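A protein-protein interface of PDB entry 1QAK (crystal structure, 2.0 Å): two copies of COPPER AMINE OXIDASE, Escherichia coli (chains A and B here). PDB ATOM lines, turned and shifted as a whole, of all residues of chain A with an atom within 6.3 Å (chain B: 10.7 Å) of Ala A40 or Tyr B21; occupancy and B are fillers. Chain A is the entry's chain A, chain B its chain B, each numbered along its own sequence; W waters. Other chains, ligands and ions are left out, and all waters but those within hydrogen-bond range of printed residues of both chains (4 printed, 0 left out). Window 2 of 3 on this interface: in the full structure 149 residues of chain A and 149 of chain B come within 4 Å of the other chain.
The backbone carbonyl oxygen of Leu B24 sits at hydrogen-bond distance from the backbone NH of Asp B19. N of Ala B22 is in hydrogen-bond range of OD1 of Asp B19. The side-chain carboxylate (OD1) of Asp B19 is in hydrogen-bond range of the backbone NH (N) of Tyr B21, 3.1 Å away. O of Lys A35 sits at hydrogen-bond distance from N of Ile A44 (2.8 Å).
3 positions are printed for both chains. Of the 9 pairs that touch across the chains among the printed residues, none has its exchanged pair printed and touching as well.
Along chain B the printed residues that touch a printed residue of chain A span positions 19 to 21. Hydrophobic or aromatic side chains of chain A within 4 Å of the printed part of chain B: Leu A24, Val A36, Ala A40 and Ile A44. Among the printed residues, Asp or Glu carboxylates within 4 Å of a Lys or Arg side-chain nitrogen of the other chain: Lys A35 with Asp B19 (2.6 Å).
Water W1 bridges OD1 of Asp B19 and NZ of Lys A35. Water W4 lies within hydrogen-bond range of O of Ala B22 (2.7 Å) and NZ of Lys A37 (3.2 Å). Water W2 lies within hydrogen-bond range of the side-chain amino group of Lys A37 (2.9 Å) and the backbone carbonyl oxygen of Tyr B21 (3.0 Å). Water W3 lies within hydrogen-bond range of the side-chain amino group (NZ) of Lys B37 (3.0 Å) and the side-chain amino group (NZ) of Lys A37 (3.5 Å).
Printed residues of chain B within 4 Å of Leu A24: Tyr B21 (3.8 Å). Printed residues of chain B within 4 Å of Lys A37: Tyr B21. Pro A38 touches none of the printed residues of chain B. No residue of chain B comes within 4 Å of Gly A39. Of chain B, only Tyr B21 comes within 4 Å of Ala A40. No residue of chain B comes within 4 Å of Gln A41. Thr A42 touches one residue of chain B. Of the printed residues of chain B, Ile A44 touches Tyr B21. No residue of chain B comes within 4 Å of Leu A52. No residue of chain B comes within 4 Å of Pro A55. Printed residues of chain A within 4 Å of Asp B19: Lys A35 (2.6 Å). Tyr B21 touches just these residues of chain A: Leu A24 (3.8 Å), Lys A35 (3.6 Å), Val A36 (3.3 Å), Lys A37 (2.9 Å), Ala A40 (3.6 Å), Thr A42 (2.6 Å), Ala A43 (3.7 Å) and Ile A44 (3.3 Å). The nearest residue of chain A that does not touch Tyr B21 is Leu A52 (5.7 Å). The nearest printed residue of chain A that does not touch Asp B19 is Ile A44 (5.6 Å).
The backbone carbonyl oxygen of Thr A42 is in hydrogen-bond range of the side-chain hydroxyl of Tyr B21 (2.6 Å). The side-chain amino group (NZ) of Lys A35 is in salt-bridge range of the side-chain carboxylate (OD2) of Asp B19 (2.6 Å). The side-chain hydroxyl (OH) of Tyr B21 lies within hydrogen-bond range of the backbone NH (N) of Lys A37 (2.9 Å).
CE2 of Tyr B21 touches CD2 of Leu A24, at 3.8 Å. O of Lys A35 touches CE2 of Tyr B21, 3.6 Å away. Tyr B21 touches Val A36. Ala A40 touches Tyr B21 (CB to OH, 3.6 Å). Ala A43 touches Tyr B21 (CA to OH, 3.7 Å). CG of Tyr B21 touches CG1 of Ile A44, 3.3 Å away.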
ATOM      1  N   LEU A  24     -20.001 -28.457 -16.495  1.00  0.00           N
ATOM      2  CA  LEU A  24     -21.109 -27.585 -16.114  1.00  0.00           C
ATOM      3  C   LEU A  24     -21.524 -27.686 -14.663  1.00  0.00           C
ATOM      4  O   LEU A  24     -21.656 -28.795 -14.129  1.00  0.00           O
ATOM      5  CB  LEU A  24     -22.277 -28.087 -16.982  1.00  0.00           C
ATOM      6  CG  LEU A  24     -23.606 -27.323 -17.147  1.00  0.00           C
ATOM      7  CD1 LEU A  24     -24.287 -27.273 -15.790  1.00  0.00           C
ATOM      8  CD2 LEU A  24     -23.435 -25.855 -17.556  1.00  0.00           C
ATOM      9  N   LYS A  35     -27.526 -22.698 -14.369  1.00  0.00           N
ATOM     10  CA  LYS A  35     -26.486 -23.461 -15.050  1.00  0.00           C
ATOM     11  C   LYS A  35     -25.353 -22.496 -15.427  1.00  0.00           C
ATOM     12  O   LYS A  35     -25.599 -21.421 -15.998  1.00  0.00           O
ATOM     13  CB  LYS A  35     -27.006 -24.165 -16.305  1.00  0.00           C
ATOM     14  CG  LYS A  35     -27.942 -25.293 -15.878  1.00  0.00           C
ATOM     15  CD  LYS A  35     -28.331 -26.051 -17.132  1.00  0.00           C
ATOM     16  CE  LYS A  35     -29.485 -25.413 -17.847  1.00  0.00           C
ATOM     17  NZ  LYS A  35     -30.195 -26.443 -18.667  1.00  0.00           N
ATOM     18  N   VAL A  36     -24.133 -22.894 -15.067  1.00  0.00           N
ATOM     19  CA  VAL A  36     -23.004 -22.017 -15.402  1.00  0.00           C
ATOM     20  C   VAL A  36     -21.747 -22.818 -15.732  1.00  0.00           C
ATOM     21  O   VAL A  36     -21.488 -23.783 -15.000  1.00  0.00           O
ATOM     22  CB  VAL A  36     -22.705 -21.001 -14.272  1.00  0.00           C
ATOM     23  CG1 VAL A  36     -22.402 -21.574 -12.892  1.00  0.00           C
ATOM     24  CG2 VAL A  36     -21.711 -19.943 -14.733  1.00  0.00           C
ATOM     25  N   LYS A  37     -21.020 -22.429 -16.784  1.00  0.00           N
ATOM     26  CA  LYS A  37     -19.774 -23.094 -17.172  1.00  0.00           C
ATOM     27  C   LYS A  37     -18.585 -22.226 -16.738  1.00  0.00           C
ATOM     28  O   LYS A  37     -18.611 -20.995 -16.869  1.00  0.00           O
ATOM     29  CB  LYS A  37     -19.596 -23.266 -18.683  1.00  0.00           C
ATOM     30  CG  LYS A  37     -20.714 -24.198 -19.140  1.00  0.00           C
ATOM     31  CD  LYS A  37     -21.146 -24.269 -20.569  1.00  0.00           C
ATOM     32  CE  LYS A  37     -20.147 -23.854 -21.628  1.00  0.00           C
ATOM     33  NZ  LYS A  37     -19.226 -24.960 -21.986  1.00  0.00           N
ATOM     34  N   PRO A  38     -17.546 -22.848 -16.215  1.00  0.00           N
ATOM     35  CA  PRO A  38     -16.331 -22.140 -15.790  1.00  0.00           C
ATOM     36  C   PRO A  38     -15.870 -21.396 -17.041  1.00  0.00           C
ATOM     37  O   PRO A  38     -15.879 -21.887 -18.171  1.00  0.00           O
ATOM     38  CB  PRO A  38     -15.272 -23.249 -15.520  1.00  0.00           C
ATOM     39  CG  PRO A  38     -16.249 -24.319 -15.061  1.00  0.00           C
ATOM     40  CD  PRO A  38     -17.418 -24.299 -16.020  1.00  0.00           C
ATOM     41  N   GLY A  39     -15.467 -20.161 -16.840  1.00  0.00           N
ATOM     42  CA  GLY A  39     -14.989 -19.258 -17.866  1.00  0.00           C
ATOM     43  C   GLY A  39     -16.038 -18.675 -18.782  1.00  0.00           C
ATOM     44  O   GLY A  39     -15.655 -17.805 -19.568  1.00  0.00           O
ATOM     45  N   ALA A  40     -17.303 -19.089 -18.745  1.00  0.00           N
ATOM     46  CA  ALA A  40     -18.307 -18.538 -19.653  1.00  0.00           C
ATOM     47  C   ALA A  40     -18.697 -17.101 -19.273  1.00  0.00           C
ATOM     48  O   ALA A  40     -18.716 -16.797 -18.086  1.00  0.00           O
ATOM     49  CB  ALA A  40     -19.582 -19.366 -19.678  1.00  0.00           C
ATOM     50  N   GLN A  41     -18.996 -16.303 -20.283  1.00  0.00           N
ATOM     51  CA  GLN A  41     -19.374 -14.901 -19.993  1.00  0.00           C
ATOM     52  C   GLN A  41     -20.845 -14.804 -19.635  1.00  0.00           C
ATOM     53  O   GLN A  41     -21.317 -13.724 -19.291  1.00  0.00           O
ATOM     54  CB  GLN A  41     -19.058 -13.999 -21.200  1.00  0.00           C
ATOM     55  CG  GLN A  41     -17.572 -13.688 -21.393  1.00  0.00           C
ATOM     56  CD  GLN A  41     -17.283 -13.046 -22.735  1.00  0.00           C
ATOM     57  OE1 GLN A  41     -18.122 -12.531 -23.467  1.00  0.00           O
ATOM     58  NE2 GLN A  41     -16.023 -13.022 -23.161  1.00  0.00           N
ATOM     59  N   THR A  42     -21.569 -15.925 -19.737  1.00  0.00           N
ATOM     60  CA  THR A  42     -22.994 -15.944 -19.417  1.00  0.00           C
ATOM     61  C   THR A  42     -23.362 -17.204 -18.643  1.00  0.00           C
ATOM     62  O   THR A  42     -22.592 -18.167 -18.563  1.00  0.00           O
ATOM     63  CB  THR A  42     -23.991 -15.833 -20.585  1.00  0.00           C
ATOM     64  OG1 THR A  42     -23.954 -17.026 -21.379  1.00  0.00           O
ATOM     65  CG2 THR A  42     -23.626 -14.722 -21.574  1.00  0.00           C
ATOM     66  N   ALA A  43     -24.546 -17.179 -18.059  1.00  0.00           N
ATOM     67  CA  ALA A  43     -25.066 -18.296 -17.270  1.00  0.00           C
ATOM     68  C   ALA A  43     -26.535 -18.459 -17.669  1.00  0.00           C
ATOM     69  O   ALA A  43     -27.047 -17.706 -18.501  1.00  0.00           O
ATOM     70  CB  ALA A  43     -24.960 -17.980 -15.778  1.00  0.00           C
ATOM     71  N   ILE A  44     -27.212 -19.460 -17.101  1.00  0.00           N
ATOM     72  CA  ILE A  44     -28.624 -19.587 -17.501  1.00  0.00           C
ATOM     73  C   ILE A  44     -29.374 -19.572 -16.171  1.00  0.00           C
ATOM     74  O   ILE A  44     -28.917 -20.273 -15.257  1.00  0.00           O
ATOM     75  CB  ILE A  44     -28.836 -20.933 -18.221  1.00  0.00           C
ATOM     76  CG1 ILE A  44     -28.144 -20.962 -19.599  1.00  0.00           C
ATOM     77  CG2 ILE A  44     -30.295 -21.386 -18.343  1.00  0.00           C
ATOM     78  CD1 ILE A  44     -28.870 -20.257 -20.725  1.00  0.00           C
ATOM     79  N   LEU A  52     -22.647 -12.264 -17.232  1.00  0.00           N
ATOM     80  CA  LEU A  52     -21.998 -12.240 -15.936  1.00  0.00           C
ATOM     81  C   LEU A  52     -20.883 -11.181 -16.017  1.00  0.00           C
ATOM     82  O   LEU A  52     -20.189 -11.151 -17.045  1.00  0.00           O
ATOM     83  CB  LEU A  52     -21.302 -13.555 -15.601  1.00  0.00           C
ATOM     84  CG  LEU A  52     -22.203 -14.800 -15.578  1.00  0.00           C
ATOM     85  CD1 LEU A  52     -21.304 -16.047 -15.534  1.00  0.00           C
ATOM     86  CD2 LEU A  52     -22.994 -14.671 -14.283  1.00  0.00           C
ATOM     87  N   VAL A  54     -18.352 -11.132 -13.968  1.00  0.00           N
ATOM     88  CA  VAL A  54     -17.128 -11.907 -13.776  1.00  0.00           C
ATOM     89  C   VAL A  54     -17.389 -13.391 -13.956  1.00  0.00           C
ATOM     90  O   VAL A  54     -18.110 -13.993 -13.177  1.00  0.00           O
ATOM     91  CB  VAL A  54     -16.679 -11.606 -12.330  1.00  0.00           C
ATOM     92  CG1 VAL A  54     -15.434 -12.360 -11.885  1.00  0.00           C
ATOM     93  CG2 VAL A  54     -16.516 -10.100 -12.129  1.00  0.00           C
ATOM     94  N   PRO A  55     -16.827 -14.020 -14.958  1.00  0.00           N
ATOM     95  CA  PRO A  55     -17.013 -15.447 -15.212  1.00  0.00           C
ATOM     96  C   PRO A  55     -16.481 -16.268 -14.042  1.00  0.00           C
ATOM     97  O   PRO A  55     -15.565 -15.805 -13.344  1.00  0.00           O
ATOM     98  CB  PRO A  55     -16.240 -15.758 -16.502  1.00  0.00           C
ATOM     99  CG  PRO A  55     -16.249 -14.365 -17.101  1.00  0.00           C
ATOM    100  CD  PRO A  55     -15.957 -13.395 -15.962  1.00  0.00           C
ATOM    101  N   VAL A  56     -17.085 -17.452 -13.857  1.00  0.00           N
ATOM    102  CA  VAL A  56     -16.651 -18.329 -12.757  1.00  0.00           C
ATOM    103  C   VAL A  56     -15.225 -18.726 -13.130  1.00  0.00           C
ATOM    104  O   VAL A  56     -15.058 -18.922 -14.331  1.00  0.00           O
ATOM    105  CB  VAL A  56     -17.526 -19.592 -12.684  1.00  0.00           C
ATOM    106  CG1 VAL A  56     -16.961 -20.704 -11.800  1.00  0.00           C
ATOM    107  CG2 VAL A  56     -18.920 -19.258 -12.167  1.00  0.00           C
ATOM    108  N   GLN B  17     -33.524 -34.372 -24.788  1.00  0.00           N
ATOM    109  CA  GLN B  17     -33.442 -33.009 -24.305  1.00  0.00           C
ATOM    110  C   GLN B  17     -32.183 -32.360 -24.870  1.00  0.00           C
ATOM    111  O   GLN B  17     -31.093 -32.946 -24.770  1.00  0.00           O
ATOM    112  CB  GLN B  17     -33.554 -32.980 -22.771  1.00  0.00           C
ATOM    113  CG  GLN B  17     -34.431 -33.928 -21.975  1.00  0.00           C
ATOM    114  CD  GLN B  17     -34.026 -35.004 -20.953  1.00  0.00           C
ATOM    115  OE1 GLN B  17     -33.800 -34.779 -19.721  1.00  0.00           O
ATOM    116  NE2 GLN B  17     -33.944 -36.275 -21.447  1.00  0.00           N
ATOM    117  N   TRP B  18     -32.343 -31.155 -25.450  1.00  0.00           N
ATOM    118  CA  TRP B  18     -31.150 -30.489 -26.005  1.00  0.00           C
ATOM    119  C   TRP B  18     -30.868 -29.236 -25.199  1.00  0.00           C
ATOM    120  O   TRP B  18     -31.815 -28.477 -25.085  1.00  0.00           O
ATOM    121  CB  TRP B  18     -31.330 -30.137 -27.475  1.00  0.00           C
ATOM    122  CG  TRP B  18     -30.314 -29.154 -27.973  1.00  0.00           C
ATOM    123  CD1 TRP B  18     -30.564 -27.871 -28.383  1.00  0.00           C
ATOM    124  CD2 TRP B  18     -28.901 -29.341 -28.118  1.00  0.00           C
ATOM    125  NE1 TRP B  18     -29.406 -27.259 -28.774  1.00  0.00           N
ATOM    126  CE2 TRP B  18     -28.365 -28.136 -28.621  1.00  0.00           C
ATOM    127  CE3 TRP B  18     -28.041 -30.414 -27.874  1.00  0.00           C
ATOM    128  CZ2 TRP B  18     -27.005 -27.968 -28.887  1.00  0.00           C
ATOM    129  CZ3 TRP B  18     -26.698 -30.225 -28.149  1.00  0.00           C
ATOM    130  CH2 TRP B  18     -26.175 -29.019 -28.650  1.00  0.00           C
ATOM    131  N   ASP B  19     -29.688 -29.033 -24.646  1.00  0.00           N
ATOM    132  CA  ASP B  19     -29.372 -27.853 -23.845  1.00  0.00           C
ATOM    133  C   ASP B  19     -28.418 -27.062 -24.731  1.00  0.00           C
ATOM    134  O   ASP B  19     -27.259 -27.450 -24.951  1.00  0.00           O
ATOM    135  CB  ASP B  19     -28.652 -28.302 -22.559  1.00  0.00           C
ATOM    136  CG  ASP B  19     -28.410 -27.142 -21.608  1.00  0.00           C
ATOM    137  OD1 ASP B  19     -28.175 -26.015 -22.081  1.00  0.00           O
ATOM    138  OD2 ASP B  19     -28.472 -27.254 -20.369  1.00  0.00           O
ATOM    139  N   ASP B  20     -28.931 -25.933 -25.232  1.00  0.00           N
ATOM    140  CA  ASP B  20     -28.126 -25.086 -26.099  1.00  0.00           C
ATOM    141  C   ASP B  20     -26.974 -24.395 -25.396  1.00  0.00           C
ATOM    142  O   ASP B  20     -25.928 -24.175 -26.000  1.00  0.00           O
ATOM    143  CB  ASP B  20     -29.107 -24.100 -26.754  1.00  0.00           C
ATOM    144  CG  ASP B  20     -28.354 -23.185 -27.693  1.00  0.00           C
ATOM    145  OD1 ASP B  20     -27.881 -23.633 -28.752  1.00  0.00           O
ATOM    146  OD2 ASP B  20     -28.273 -22.025 -27.259  1.00  0.00           O
ATOM    147  N   TYR B  21     -27.104 -24.014 -24.141  1.00  0.00           N
ATOM    148  CA  TYR B  21     -26.030 -23.347 -23.411  1.00  0.00           C
ATOM    149  C   TYR B  21     -24.892 -24.333 -23.157  1.00  0.00           C
ATOM    150  O   TYR B  21     -23.738 -24.011 -23.367  1.00  0.00           O
ATOM    151  CB  TYR B  21     -26.533 -22.894 -22.033  1.00  0.00           C
ATOM    152  CG  TYR B  21     -25.485 -22.292 -21.122  1.00  0.00           C
ATOM    153  CD1 TYR B  21     -24.889 -21.055 -21.370  1.00  0.00           C
ATOM    154  CD2 TYR B  21     -25.115 -23.015 -19.985  1.00  0.00           C
ATOM    155  CE1 TYR B  21     -23.945 -20.560 -20.487  1.00  0.00           C
ATOM    156  CE2 TYR B  21     -24.175 -22.509 -19.113  1.00  0.00           C
ATOM    157  CZ  TYR B  21     -23.579 -21.286 -19.359  1.00  0.00           C
ATOM    158  OH  TYR B  21     -22.641 -20.795 -18.479  1.00  0.00           O
ATOM    159  N   ALA B  22     -25.207 -25.543 -22.695  1.00  0.00           N
ATOM    160  CA  ALA B  22     -24.210 -26.559 -22.403  1.00  0.00           C
ATOM    161  C   ALA B  22     -23.802 -27.331 -23.657  1.00  0.00           C
ATOM    162  O   ALA B  22     -22.826 -28.081 -23.528  1.00  0.00           O
ATOM    163  CB  ALA B  22     -24.905 -27.525 -21.414  1.00  0.00           C
ATOM    164  N   GLN B  23     -24.492 -27.178 -24.787  1.00  0.00           N
ATOM    165  CA  GLN B  23     -24.147 -27.899 -25.996  1.00  0.00           C
ATOM    166  C   GLN B  23     -24.211 -29.391 -25.663  1.00  0.00           C
ATOM    167  O   GLN B  23     -23.369 -30.236 -26.002  1.00  0.00           O
ATOM    168  CB  GLN B  23     -22.851 -27.549 -26.728  1.00  0.00           C
ATOM    169  CG  GLN B  23     -22.840 -26.062 -27.135  1.00  0.00           C
ATOM    170  CD  GLN B  23     -23.757 -25.915 -28.340  1.00  0.00           C
ATOM    171  OE1 GLN B  23     -23.397 -26.586 -29.299  1.00  0.00           O
ATOM    172  NE2 GLN B  23     -24.839 -25.129 -28.316  1.00  0.00           N
ATOM    173  N   LEU B  24     -25.318 -29.699 -24.971  1.00  0.00           N
ATOM    174  CA  LEU B  24     -25.526 -31.071 -24.533  1.00  0.00           C
ATOM    175  C   LEU B  24     -26.882 -31.725 -24.734  1.00  0.00           C
ATOM    176  O   LEU B  24     -27.943 -31.139 -24.546  1.00  0.00           O
ATOM    177  CB  LEU B  24     -25.267 -30.996 -22.997  1.00  0.00           C
ATOM    178  CG  LEU B  24     -25.298 -32.330 -22.218  1.00  0.00           C
ATOM    179  CD1 LEU B  24     -23.973 -33.062 -22.299  1.00  0.00           C
ATOM    180  CD2 LEU B  24     -25.562 -32.046 -20.736  1.00  0.00           C
ATOM    181  N   PHE B  25     -26.848 -33.002 -25.121  1.00  0.00           N
ATOM    182  CA  PHE B  25     -28.110 -33.713 -25.292  1.00  0.00           C
ATOM    183  C   PHE B  25     -28.194 -34.619 -24.048  1.00  0.00           C
ATOM    184  O   PHE B  25     -27.173 -35.172 -23.612  1.00  0.00           O
ATOM    185  CB  PHE B  25     -28.081 -34.666 -26.483  1.00  0.00           C
ATOM    186  CG  PHE B  25     -28.392 -34.077 -27.824  1.00  0.00           C
ATOM    187  CD1 PHE B  25     -29.714 -33.776 -28.125  1.00  0.00           C
ATOM    188  CD2 PHE B  25     -27.379 -33.832 -28.744  1.00  0.00           C
ATOM    189  CE1 PHE B  25     -30.075 -33.220 -29.341  1.00  0.00           C
ATOM    190  CE2 PHE B  25     -27.737 -33.269 -29.974  1.00  0.00           C
ATOM    191  CZ  PHE B  25     -29.056 -32.973 -30.257  1.00  0.00           C
ATOM    192  N   LYS B  37     -22.448 -34.932 -25.987  1.00  0.00           N
ATOM    193  CA  LYS B  37     -22.207 -33.626 -26.601  1.00  0.00           C
ATOM    194  C   LYS B  37     -21.874 -33.833 -28.067  1.00  0.00           C
ATOM    195  O   LYS B  37     -21.111 -34.748 -28.408  1.00  0.00           O
ATOM    196  CB  LYS B  37     -20.975 -32.989 -25.947  1.00  0.00           C
ATOM    197  CG  LYS B  37     -21.145 -32.557 -24.500  1.00  0.00           C
ATOM    198  CD  LYS B  37     -19.797 -32.241 -23.906  1.00  0.00           C
ATOM    199  CE  LYS B  37     -19.145 -30.954 -24.356  1.00  0.00           C
ATOM    200  NZ  LYS B  37     -20.149 -29.912 -24.697  1.00  0.00           N
ATOM    201  N   PRO B  38     -22.384 -33.041 -28.994  1.00  0.00           N
ATOM    202  CA  PRO B  38     -22.060 -33.207 -30.412  1.00  0.00           C
ATOM    203  C   PRO B  38     -20.541 -33.189 -30.529  1.00  0.00           C
ATOM    204  O   PRO B  38     -19.909 -32.528 -29.715  1.00  0.00           O
ATOM    205  CB  PRO B  38     -22.589 -31.949 -31.145  1.00  0.00           C
ATOM    206  CG  PRO B  38     -23.597 -31.437 -30.150  1.00  0.00           C
ATOM    207  CD  PRO B  38     -23.297 -31.924 -28.752  1.00  0.00           C
ATOM    208  N   MET B  58     -23.557 -32.507 -35.551  1.00  0.00           N
ATOM    209  CA  MET B  58     -24.532 -31.414 -35.644  1.00  0.00           C
ATOM    210  C   MET B  58     -24.374 -30.785 -37.020  1.00  0.00           C
ATOM    211  O   MET B  58     -23.312 -30.276 -37.366  1.00  0.00           O
ATOM    212  CB  MET B  58     -24.350 -30.488 -34.453  1.00  0.00           C
ATOM    213  CG  MET B  58     -25.480 -29.483 -34.333  1.00  0.00           C
ATOM    214  SD  MET B  58     -27.019 -30.270 -33.809  1.00  0.00           S
ATOM    215  CE  MET B  58     -27.978 -28.837 -33.357  1.00  0.00           C
HETATM  216  O   HOH W   1     -29.727 -24.188 -20.858  1.00  0.00           O
HETATM  217  O   HOH W   2     -21.051 -25.100 -24.248  1.00  0.00           O
HETATM  218  O   HOH W   3     -19.553 -26.938 -24.845  1.00  0.00           O
HETATM  219  O   HOH W   4     -20.634 -27.822 -21.897  1.00  0.00           O
